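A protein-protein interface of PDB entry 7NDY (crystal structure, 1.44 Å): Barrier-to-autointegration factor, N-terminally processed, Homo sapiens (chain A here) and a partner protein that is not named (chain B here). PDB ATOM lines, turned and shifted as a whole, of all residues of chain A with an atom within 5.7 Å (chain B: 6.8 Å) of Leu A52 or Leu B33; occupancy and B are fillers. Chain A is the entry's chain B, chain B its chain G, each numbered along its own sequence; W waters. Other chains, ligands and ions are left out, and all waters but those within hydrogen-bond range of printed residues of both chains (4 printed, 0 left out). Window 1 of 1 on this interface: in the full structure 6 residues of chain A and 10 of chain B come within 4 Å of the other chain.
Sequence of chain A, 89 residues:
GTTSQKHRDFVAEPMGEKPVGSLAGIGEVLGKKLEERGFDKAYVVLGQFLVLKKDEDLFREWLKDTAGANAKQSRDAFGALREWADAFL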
ATOM      1  N   GLY A  47     -18.248 -23.910  26.279  1.00  0.00           N
ATOM      2  CA  GLY A  47     -16.838 -23.804  26.646  1.00  0.00           C
ATOM      3  C   GLY A  47     -15.947 -23.853  25.418  1.00  0.00           C
ATOM      4  O   GLY A  47     -15.103 -22.982  25.246  1.00  0.00           O
ATOM      5  N   GLN A  48     -16.247 -24.780  24.503  1.00  0.00           N
ATOM      6  CA  GLN A  48     -15.478 -24.934  23.265  1.00  0.00           C
ATOM      7  C   GLN A  48     -15.663 -23.691  22.391  1.00  0.00           C
ATOM      8  O   GLN A  48     -14.687 -23.142  21.922  1.00  0.00           O
ATOM      9  CB  GLN A  48     -15.904 -26.201  22.510  1.00  0.00           C
ATOM     10  CG  GLN A  48     -15.043 -26.473  21.291  1.00  0.00           C
ATOM     11  CD  GLN A  48     -13.686 -27.052  21.630  1.00  0.00           C
ATOM     12  OE1 GLN A  48     -13.293 -27.255  22.810  1.00  0.00           O
ATOM     13  NE2 GLN A  48     -12.918 -27.339  20.588  1.00  0.00           N
ATOM     14  N   PHE A  49     -16.896 -23.227  22.194  1.00  0.00           N
ATOM     15  CA  PHE A  49     -17.176 -21.976  21.477  1.00  0.00           C
ATOM     16  C   PHE A  49     -16.354 -20.786  22.070  1.00  0.00           C
ATOM     17  O   PHE A  49     -15.803 -19.983  21.309  1.00  0.00           O
ATOM     18  CB  PHE A  49     -18.705 -21.692  21.535  1.00  0.00           C
ATOM     19  CG  PHE A  49     -19.219 -20.279  21.333  1.00  0.00           C
ATOM     20  CD1 PHE A  49     -19.614 -19.838  20.078  1.00  0.00           C
ATOM     21  CD2 PHE A  49     -19.422 -19.436  22.415  1.00  0.00           C
ATOM     22  CE1 PHE A  49     -20.105 -18.542  19.904  1.00  0.00           C
ATOM     23  CE2 PHE A  49     -19.928 -18.158  22.242  1.00  0.00           C
ATOM     24  CZ  PHE A  49     -20.281 -17.723  20.988  1.00  0.00           C
ATOM     25  N   LEU A  50     -16.238 -20.721  23.403  1.00  0.00           N
ATOM     26  CA  LEU A  50     -15.500 -19.663  24.104  1.00  0.00           C
ATOM     27  C   LEU A  50     -13.981 -19.811  23.945  1.00  0.00           C
ATOM     28  O   LEU A  50     -13.297 -18.811  23.668  1.00  0.00           O
ATOM     29  CB  LEU A  50     -15.891 -19.615  25.588  1.00  0.00           C
ATOM     30  CG  LEU A  50     -17.333 -19.248  25.903  1.00  0.00           C
ATOM     31  CD1 LEU A  50     -17.560 -19.227  27.406  1.00  0.00           C
ATOM     32  CD2 LEU A  50     -17.717 -17.909  25.284  1.00  0.00           C
ATOM     33  N   VAL A  51     -13.438 -21.046  24.079  1.00  0.00           N
ATOM     34  CA  VAL A  51     -11.982 -21.237  23.868  1.00  0.00           C
ATOM     35  C   VAL A  51     -11.591 -20.984  22.410  1.00  0.00           C
ATOM     36  O   VAL A  51     -10.443 -20.658  22.156  1.00  0.00           O
ATOM     37  CB  VAL A  51     -11.358 -22.570  24.370  1.00  0.00           C
ATOM     38  CG1 VAL A  51     -11.651 -22.824  25.815  1.00  0.00           C
ATOM     39  CG2 VAL A  51     -11.753 -23.759  23.518  1.00  0.00           C
ATOM     40  N   LEU A  52     -12.539 -21.125  21.463  1.00  0.00           N
ATOM     41  CA  LEU A  52     -12.370 -20.806  20.036  1.00  0.00           C
ATOM     42  C   LEU A  52     -12.676 -19.286  19.792  1.00  0.00           C
ATOM     43  O   LEU A  52     -12.912 -18.889  18.661  1.00  0.00           O
ATOM     44  CB  LEU A  52     -13.317 -21.701  19.180  1.00  0.00           C
ATOM     45  CG  LEU A  52     -12.971 -23.199  19.183  1.00  0.00           C
ATOM     46  CD1 LEU A  52     -13.989 -24.024  18.395  1.00  0.00           C
ATOM     47  CD2 LEU A  52     -11.541 -23.446  18.658  1.00  0.00           C
ATOM     48  N   LYS A  53     -12.711 -18.448  20.868  1.00  0.00           N
ATOM     49  CA  LYS A  53     -12.919 -16.990  20.840  1.00  0.00           C
ATOM     50  C   LYS A  53     -14.179 -16.603  20.070  1.00  0.00           C
ATOM     51  O   LYS A  53     -14.172 -15.611  19.351  1.00  0.00           O
ATOM     52  CB  LYS A  53     -11.689 -16.282  20.251  1.00  0.00           C
ATOM     53  CG  LYS A  53     -10.497 -16.335  21.199  1.00  0.00           C
ATOM     54  CD  LYS A  53      -9.531 -15.199  20.941  1.00  0.00           C
ATOM     55  CE  LYS A  53     -10.120 -13.798  21.040  1.00  0.00           C
ATOM     56  NZ  LYS A  53     -10.903 -13.573  22.300  1.00  0.00           N
ATOM     57  N   LYS A  54     -15.235 -17.421  20.187  1.00  0.00           N
ATOM     58  CA  LYS A  54     -16.517 -17.195  19.487  1.00  0.00           C
ATOM     59  C   LYS A  54     -16.315 -17.092  17.967  1.00  0.00           C
ATOM     60  O   LYS A  54     -17.119 -16.459  17.305  1.00  0.00           O
ATOM     61  CB  LYS A  54     -17.215 -15.924  19.998  1.00  0.00           C
ATOM     62  CG  LYS A  54     -17.224 -15.807  21.519  1.00  0.00           C
ATOM     63  CD  LYS A  54     -17.878 -14.510  21.927  1.00  0.00           C
ATOM     64  CE  LYS A  54     -17.822 -14.254  23.406  1.00  0.00           C
ATOM     65  NZ  LYS A  54     -18.200 -12.843  23.693  1.00  0.00           N
ATOM     66  N   ASP A  55     -15.268 -17.710  17.427  1.00  0.00           N
ATOM     67  CA  ASP A  55     -14.995 -17.664  15.997  1.00  0.00           C
ATOM     68  C   ASP A  55     -15.898 -18.656  15.249  1.00  0.00           C
ATOM     69  O   ASP A  55     -15.774 -19.863  15.436  1.00  0.00           O
ATOM     70  CB  ASP A  55     -13.523 -17.987  15.757  1.00  0.00           C
ATOM     71  CG  ASP A  55     -13.080 -17.784  14.336  1.00  0.00           C
ATOM     72  OD1 ASP A  55     -13.497 -18.573  13.471  1.00  0.00           O
ATOM     73  OD2 ASP A  55     -12.306 -16.837  14.087  1.00  0.00           O
ATOM     74  N   LEU A  58     -13.879 -21.383  13.115  1.00  0.00           N
ATOM     75  CA  LEU A  58     -13.252 -22.397  13.976  1.00  0.00           C
ATOM     76  C   LEU A  58     -14.296 -23.322  14.598  1.00  0.00           C
ATOM     77  O   LEU A  58     -14.117 -24.539  14.589  1.00  0.00           O
ATOM     78  CB  LEU A  58     -12.427 -21.723  15.083  1.00  0.00           C
ATOM     79  CG  LEU A  58     -11.206 -20.997  14.604  1.00  0.00           C
ATOM     80  CD1 LEU A  58     -10.591 -20.191  15.720  1.00  0.00           C
ATOM     81  CD2 LEU A  58     -10.186 -21.969  14.003  1.00  0.00           C
ATOM     82  N   PHE A  59     -15.396 -22.750  15.138  1.00  0.00           N
ATOM     83  CA  PHE A  59     -16.417 -23.558  15.771  1.00  0.00           C
ATOM     84  C   PHE A  59     -17.063 -24.535  14.811  1.00  0.00           C
ATOM     85  O   PHE A  59     -17.225 -25.713  15.136  1.00  0.00           O
ATOM     86  CB  PHE A  59     -17.477 -22.691  16.468  1.00  0.00           C
ATOM     87  CG  PHE A  59     -18.551 -23.501  17.137  1.00  0.00           C
ATOM     88  CD1 PHE A  59     -18.388 -23.962  18.431  1.00  0.00           C
ATOM     89  CD2 PHE A  59     -19.710 -23.850  16.453  1.00  0.00           C
ATOM     90  CE1 PHE A  59     -19.367 -24.737  19.034  1.00  0.00           C
ATOM     91  CE2 PHE A  59     -20.688 -24.616  17.067  1.00  0.00           C
ATOM     92  CZ  PHE A  59     -20.501 -25.071  18.341  1.00  0.00           C
ATOM     93  N   GLU A  61     -15.899 -25.669  11.929  1.00  0.00           N
ATOM     94  CA  GLU A  61     -14.903 -26.643  11.483  1.00  0.00           C
ATOM     95  C   GLU A  61     -14.718 -27.710  12.575  1.00  0.00           C
ATOM     96  O   GLU A  61     -14.754 -28.899  12.268  1.00  0.00           O
ATOM     97  CB  GLU A  61     -13.587 -25.938  11.178  1.00  0.00           C
ATOM     98  CG  GLU A  61     -12.515 -26.833  10.595  1.00  0.00           C
ATOM     99  CD  GLU A  61     -11.349 -26.077   9.982  1.00  0.00           C
ATOM    100  OE1 GLU A  61     -10.583 -26.700   9.213  1.00  0.00           O
ATOM    101  OE2 GLU A  61     -11.203 -24.861  10.260  1.00  0.00           O
ATOM    102  N   TRP A  62     -14.553 -27.291  13.841  1.00  0.00           N
ATOM    103  CA  TRP A  62     -14.438 -28.219  14.968  1.00  0.00           C
ATOM    104  C   TRP A  62     -15.676 -29.159  15.055  1.00  0.00           C
ATOM    105  O   TRP A  62     -15.523 -30.354  15.312  1.00  0.00           O
ATOM    106  CB  TRP A  62     -14.221 -27.443  16.289  1.00  0.00           C
ATOM    107  CG  TRP A  62     -14.472 -28.278  17.510  1.00  0.00           C
ATOM    108  CD1 TRP A  62     -13.664 -29.257  18.016  1.00  0.00           C
ATOM    109  CD2 TRP A  62     -15.713 -28.384  18.205  1.00  0.00           C
ATOM    110  NE1 TRP A  62     -14.298 -29.910  19.042  1.00  0.00           N
ATOM    111  CE2 TRP A  62     -15.555 -29.381  19.192  1.00  0.00           C
ATOM    112  CE3 TRP A  62     -16.914 -27.662  18.163  1.00  0.00           C
ATOM    113  CZ2 TRP A  62     -16.573 -29.717  20.075  1.00  0.00           C
ATOM    114  CZ3 TRP A  62     -17.908 -27.974  19.072  1.00  0.00           C
ATOM    115  CH2 TRP A  62     -17.734 -28.995  20.005  1.00  0.00           C
ATOM    116  N   ASP A  65     -15.670 -31.798  12.342  1.00  0.00           N
ATOM    117  CA  ASP A  65     -14.652 -32.817  12.610  1.00  0.00           C
ATOM    118  C   ASP A  65     -14.981 -33.711  13.784  1.00  0.00           C
ATOM    119  O   ASP A  65     -14.570 -34.871  13.814  1.00  0.00           O
ATOM    120  CB  ASP A  65     -13.304 -32.158  12.859  1.00  0.00           C
ATOM    121  CG  ASP A  65     -12.771 -31.362  11.684  1.00  0.00           C
ATOM    122  OD1 ASP A  65     -13.263 -31.576  10.544  1.00  0.00           O
ATOM    123  OD2 ASP A  65     -11.877 -30.516  11.902  1.00  0.00           O
ATOM    124  N   LEU B  12       2.967 -24.405  18.663  1.00  0.00           N
ATOM    125  CA  LEU B  12       1.813 -24.592  17.793  1.00  0.00           C
ATOM    126  C   LEU B  12       1.132 -23.229  17.592  1.00  0.00           C
ATOM    127  O   LEU B  12       0.862 -22.834  16.457  1.00  0.00           O
ATOM    128  CB  LEU B  12       0.827 -25.617  18.386  1.00  0.00           C
ATOM    129  CG  LEU B  12      -0.112 -26.221  17.344  1.00  0.00           C
ATOM    130  CD1 LEU B  12       0.658 -27.151  16.393  1.00  0.00           C
ATOM    131  CD2 LEU B  12      -1.259 -26.962  17.997  1.00  0.00           C
ATOM    132  N   LEU B  16       0.498 -20.998  14.043  1.00  0.00           N
ATOM    133  CA  LEU B  16      -0.802 -20.461  13.635  1.00  0.00           C
ATOM    134  C   LEU B  16      -0.722 -18.955  13.388  1.00  0.00           C
ATOM    135  O   LEU B  16      -1.307 -18.470  12.428  1.00  0.00           O
ATOM    136  CB  LEU B  16      -1.867 -20.741  14.695  1.00  0.00           C
ATOM    137  CG  LEU B  16      -2.133 -22.210  14.890  1.00  0.00           C
ATOM    138  CD1 LEU B  16      -2.527 -22.496  16.325  1.00  0.00           C
ATOM    139  CD2 LEU B  16      -3.127 -22.738  13.832  1.00  0.00           C
ATOM    140  N   HIS B  23      -7.041 -18.037  15.253  1.00  0.00           N
ATOM    141  CA  HIS B  23      -7.013 -19.041  16.293  1.00  0.00           C
ATOM    142  C   HIS B  23      -7.192 -18.454  17.676  1.00  0.00           C
ATOM    143  O   HIS B  23      -6.858 -17.299  17.930  1.00  0.00           O
ATOM    144  CB  HIS B  23      -5.638 -19.753  16.242  1.00  0.00           C
ATOM    145  CG  HIS B  23      -4.479 -18.843  16.561  1.00  0.00           C
ATOM    146  ND1 HIS B  23      -4.040 -17.885  15.663  1.00  0.00           N
ATOM    147  CD2 HIS B  23      -3.735 -18.759  17.687  1.00  0.00           C
ATOM    148  CE1 HIS B  23      -3.043 -17.257  16.267  1.00  0.00           C
ATOM    149  NE2 HIS B  23      -2.815 -17.759  17.484  1.00  0.00           N
ATOM    150  N   GLY B  24      -7.581 -19.320  18.585  1.00  0.00           N
ATOM    151  CA  GLY B  24      -7.624 -19.042  20.010  1.00  0.00           C
ATOM    152  C   GLY B  24      -6.557 -19.902  20.688  1.00  0.00           C
ATOM    153  O   GLY B  24      -5.700 -20.535  20.042  1.00  0.00           O
ATOM    154  N   PRO B  25      -6.634 -20.022  22.005  1.00  0.00           N
ATOM    155  CA  PRO B  25      -5.698 -20.898  22.736  1.00  0.00           C
ATOM    156  C   PRO B  25      -5.600 -22.355  22.271  1.00  0.00           C
ATOM    157  O   PRO B  25      -6.585 -22.958  21.838  1.00  0.00           O
ATOM    158  CB  PRO B  25      -6.279 -20.878  24.143  1.00  0.00           C
ATOM    159  CG  PRO B  25      -6.873 -19.594  24.259  1.00  0.00           C
ATOM    160  CD  PRO B  25      -7.567 -19.374  22.935  1.00  0.00           C
ATOM    161  N   SER B  29      -8.774 -29.600  24.084  1.00  0.00           N
ATOM    162  CA  SER B  29      -9.906 -29.721  23.163  1.00  0.00           C
ATOM    163  C   SER B  29      -9.703 -29.029  21.798  1.00  0.00           C
ATOM    164  O   SER B  29     -10.581 -29.123  20.921  1.00  0.00           O
ATOM    165  CB  SER B  29     -11.190 -29.212  23.817  1.00  0.00           C
ATOM    166  OG  SER B  29     -11.151 -27.798  23.994  1.00  0.00           O
ATOM    167  N   THR B  30      -8.596 -28.276  21.630  1.00  0.00           N
ATOM    168  CA  THR B  30      -8.366 -27.593  20.336  1.00  0.00           C
ATOM    169  C   THR B  30      -7.108 -28.046  19.607  1.00  0.00           C
ATOM    170  O   THR B  30      -6.928 -27.702  18.430  1.00  0.00           O
ATOM    171  CB  THR B  30      -8.381 -26.079  20.473  1.00  0.00           C
ATOM    172  OG1 THR B  30      -7.274 -25.714  21.269  1.00  0.00           O
ATOM    173  CG2 THR B  30      -9.667 -25.552  21.121  1.00  0.00           C
ATOM    174  N   ARG B  31      -6.217 -28.770  20.300  1.00  0.00           N
ATOM    175  CA  ARG B  31      -4.958 -29.255  19.743  1.00  0.00           C
ATOM    176  C   ARG B  31      -5.160 -29.977  18.394  1.00  0.00           C
ATOM    177  O   ARG B  31      -4.563 -29.578  17.388  1.00  0.00           O
ATOM    178  CB  ARG B  31      -4.273 -30.168  20.771  1.00  0.00           C
ATOM    179  CG  ARG B  31      -2.965 -30.750  20.283  1.00  0.00           C
ATOM    180  CD  ARG B  31      -1.793 -29.875  20.675  1.00  0.00           C
ATOM    181  NE  ARG B  31      -0.598 -30.261  19.920  1.00  0.00           N
ATOM    182  CZ  ARG B  31       0.600 -29.717  20.076  1.00  0.00           C
ATOM    183  NH1 ARG B  31       0.793 -28.765  20.981  1.00  0.00           N
ATOM    184  NH2 ARG B  31       1.627 -30.142  19.349  1.00  0.00           N
ATOM    185  N   ARG B  32      -6.060 -30.971  18.360  1.00  0.00           N
ATOM    186  CA  ARG B  32      -6.324 -31.729  17.136  1.00  0.00           C
ATOM    187  C   ARG B  32      -6.783 -30.846  15.975  1.00  0.00           C
ATOM    188  O   ARG B  32      -6.342 -31.013  14.832  1.00  0.00           O
ATOM    189  CB  ARG B  32      -7.313 -32.864  17.414  1.00  0.00           C
ATOM    190  CG  ARG B  32      -7.679 -33.706  16.198  1.00  0.00           C
ATOM    191  CD  ARG B  32      -8.707 -34.740  16.601  1.00  0.00           C
ATOM    192  NE  ARG B  32      -9.106 -35.614  15.495  1.00  0.00           N
ATOM    193  CZ  ARG B  32      -9.805 -36.737  15.650  1.00  0.00           C
ATOM    194  NH1 ARG B  32     -10.179 -37.136  16.864  1.00  0.00           N
ATOM    195  NH2 ARG B  32     -10.119 -37.480  14.596  1.00  0.00           N
ATOM    196  N   LEU B  33      -7.619 -29.861  16.290  1.00  0.00           N
ATOM    197  CA  LEU B  33      -8.130 -28.936  15.280  1.00  0.00           C
ATOM    198  C   LEU B  33      -6.990 -28.110  14.660  1.00  0.00           C
ATOM    199  O   LEU B  33      -6.891 -28.003  13.441  1.00  0.00           O
ATOM    200  CB  LEU B  33      -9.175 -28.015  15.957  1.00  0.00           C
ATOM    201  CG  LEU B  33      -9.682 -26.884  15.094  1.00  0.00           C
ATOM    202  CD1 LEU B  33     -10.495 -27.436  13.939  1.00  0.00           C
ATOM    203  CD2 LEU B  33     -10.466 -25.866  15.919  1.00  0.00           C
ATOM    204  N   TYR B  34      -6.143 -27.520  15.497  1.00  0.00           N
ATOM    205  CA  TYR B  34      -5.080 -26.661  15.020  1.00  0.00           C
ATOM    206  C   TYR B  34      -4.006 -27.450  14.283  1.00  0.00           C
ATOM    207  O   TYR B  34      -3.486 -26.968  13.296  1.00  0.00           O
ATOM    208  CB  TYR B  34      -4.527 -25.824  16.172  1.00  0.00           C
ATOM    209  CG  TYR B  34      -5.545 -24.808  16.636  1.00  0.00           C
ATOM    210  CD1 TYR B  34      -6.170 -23.950  15.729  1.00  0.00           C
ATOM    211  CD2 TYR B  34      -5.854 -24.671  17.983  1.00  0.00           C
ATOM    212  CE1 TYR B  34      -7.113 -23.017  16.147  1.00  0.00           C
ATOM    213  CE2 TYR B  34      -6.769 -23.724  18.416  1.00  0.00           C
ATOM    214  CZ  TYR B  34      -7.427 -22.924  17.492  1.00  0.00           C
ATOM    215  OH  TYR B  34      -8.295 -21.957  17.918  1.00  0.00           O
ATOM    216  N   GLU B  35      -3.732 -28.696  14.711  1.00  0.00           N
ATOM    217  CA  GLU B  35      -2.766 -29.535  13.995  1.00  0.00           C
ATOM    218  C   GLU B  35      -3.316 -29.874  12.600  1.00  0.00           C
ATOM    219  O   GLU B  35      -2.570 -29.867  11.615  1.00  0.00           O
ATOM    220  CB  GLU B  35      -2.498 -30.817  14.786  1.00  0.00           C
ATOM    221  CG  GLU B  35      -1.558 -30.597  15.957  1.00  0.00           C
ATOM    222  CD  GLU B  35      -0.905 -31.857  16.487  1.00  0.00           C
ATOM    223  OE1 GLU B  35      -0.302 -31.791  17.581  1.00  0.00           O
ATOM    224  OE2 GLU B  35      -0.986 -32.907  15.809  1.00  0.00           O
ATOM    225  N   LYS B  36      -4.607 -30.173  12.511  1.00  0.00           N
ATOM    226  CA  LYS B  36      -5.246 -30.501  11.233  1.00  0.00           C
ATOM    227  C   LYS B  36      -5.210 -29.286  10.313  1.00  0.00           C
ATOM    228  O   LYS B  36      -4.778 -29.394   9.153  1.00  0.00           O
ATOM    229  CB  LYS B  36      -6.678 -30.978  11.478  1.00  0.00           C
ATOM    230  CG  LYS B  36      -7.430 -31.260  10.202  1.00  0.00           C
ATOM    231  CD  LYS B  36      -8.906 -31.012  10.385  1.00  0.00           C
ATOM    232  CE  LYS B  36      -9.220 -29.547  10.241  1.00  0.00           C
ATOM    233  NZ  LYS B  36     -10.637 -29.340   9.812  1.00  0.00           N
ATOM    234  N   LYS B  37      -5.542 -28.111  10.861  1.00  0.00           N
ATOM    235  CA  LYS B  37      -5.520 -26.862  10.100  1.00  0.00           C
ATOM    236  C   LYS B  37      -4.116 -26.521   9.589  1.00  0.00           C
ATOM    237  O   LYS B  37      -3.951 -26.134   8.428  1.00  0.00           O
ATOM    238  CB  LYS B  37      -6.073 -25.730  10.966  1.00  0.00           C
ATOM    239  CG  LYS B  37      -7.582 -25.851  11.172  1.00  0.00           C
ATOM    240  CD  LYS B  37      -8.055 -24.921  12.247  1.00  0.00           C
ATOM    241  CE  LYS B  37      -7.867 -23.505  11.785  1.00  0.00           C
ATOM    242  NZ  LYS B  37      -8.766 -23.183  10.634  1.00  0.00           N
ATOM    243  N   ILE B  38      -3.096 -26.694  10.439  1.00  0.00           N
ATOM    244  CA  ILE B  38      -1.722 -26.456  10.034  1.00  0.00           C
ATOM    245  C   ILE B  38      -1.326 -27.404   8.884  1.00  0.00           C
ATOM    246  O   ILE B  38      -0.802 -26.936   7.860  1.00  0.00           O
ATOM    247  CB  ILE B  38      -0.784 -26.526  11.263  1.00  0.00           C
ATOM    248  CG1 ILE B  38      -0.925 -25.241  12.082  1.00  0.00           C
ATOM    249  CG2 ILE B  38       0.661 -26.732  10.835  1.00  0.00           C
ATOM    250  CD1 ILE B  38      -0.388 -25.332  13.393  1.00  0.00           C
HETATM  251  O   HOH W   1      -8.860 -22.070  20.581  1.00  0.00           O
HETATM  252  O   HOH W   2     -11.948 -22.237   9.586  1.00  0.00           O
HETATM  253  O   HOH W   3     -13.653 -29.656   8.749  1.00  0.00           O
HETATM  254  O   HOH W   4     -12.365 -31.299  20.876  1.00  0.00           O
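Water W1 lies within hydrogen-bond range of O of Val A51 (2.6 Å), OH of Tyr B34 (2.7 Å) and O of Pro B25 (2.7 Å). Water W3 lies within hydrogen-bond range of OD1 of Asp A65 and NZ of Lys B36. Water W2 bridges OE2 of Glu A61 (2.8 Å) and NZ of Lys B37 (3.5 Å). Water W4 bridges the backbone carbonyl oxygen of Ser B29 and the indole nitrogen of Trp A62.
The indole nitrogen (NE1) of Trp A62 sits close to the side-chain amide nitrogen (NE2) of Gln A48. The backbone NH of Leu A58 sits at hydrogen-bond distance from the side-chain carboxylate of Asp A55, at 2.9 Å. The backbone NH (N) of Gly B24 is in hydrogen-bond range of the side-chain hydroxyl (OH) of Tyr B34. O of Pro B25 lies within hydrogen-bond range of OG1 of Thr B30.
Among the printed residues, pairs that only touch across the chains: Val A51 with Pro B25 (3.2 Å), Leu A58 with Lys B37 (3.6 Å), Leu A58 with Tyr B34 (3.6 Å), Leu A52 with Tyr B34 (3.6 Å), Val A51 with Thr B30 (3.6 Å), Leu A52 with Thr B30 (3.7 Å), Gln A48 with Thr B30 (3.7 Å), Leu A58 with His B23 (3.8 Å), Leu A52 with Leu B33 (3.8 Å), Val A51 with Gly B24 (3.9 Å), Asp A65 with Leu B33 (3.9 Å) and Glu A61 with Leu B33 (3.95 Å).
Phe A49 touches none of the printed residues of chain B. Of the printed residues of chain B, Val A51 touches Gly B24 (3.9 Å), Pro B25 (3.2 Å) and Thr B30 (3.6 Å). Leu A52 touches just these residues of chain B: Thr B30, Leu B33 and Tyr B34. Trp A62 touches none of the printed residues of chain B. Printed residues of chain B within 4 Å of Asp A65: Leu B33 and Lys B36. Of the printed residues of chain A, Gly B24 touches Val A51 (3.9 Å). Leu B33 touches three residues of chain A. The nearest printed residue of chain A that does not touch Lys B37 is Asp A65 (6.4 Å).
Of the 14 printed residues of chain A, 6 touch a printed residue of chain B. Hydrophobic or aromatic side chains of chain A that line the printed part of chain B: Val A51, Leu A52 and Leu A58. Of the 15 printed residues of chain B, 9 touch a printed residue of chain A. Hydrophobic or aromatic side chains of chain B within 4 Å of the printed part of chain A: Pro B25, Leu B33 and Tyr B34. Among the printed residues, 16 pairs touch across the chains. Among the printed residues, Asp or Glu carboxylates within 4 Å of a Lys or Arg side-chain nitrogen of the other chain: Glu A61 with Lys B36, Glu A61 with Lys B37 and Asp A65 with Lys B36.
The side-chain hydroxyl (OG) of Ser B29 is in hydrogen-bond range of the side-chain amide oxygen (OE1) of Gln A48 (2.5 Å). The side-chain carboxylate of Glu A61 is in salt-bridge range of the side-chain amino group of Lys B36 (2.7 Å). OE2 of Glu A61 lies within salt-bridge range of NZ of Lys B37 (3.0 Å). OD2 of Asp A65 lies within salt-bridge range of NZ of Lys B36 (2.7 Å).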
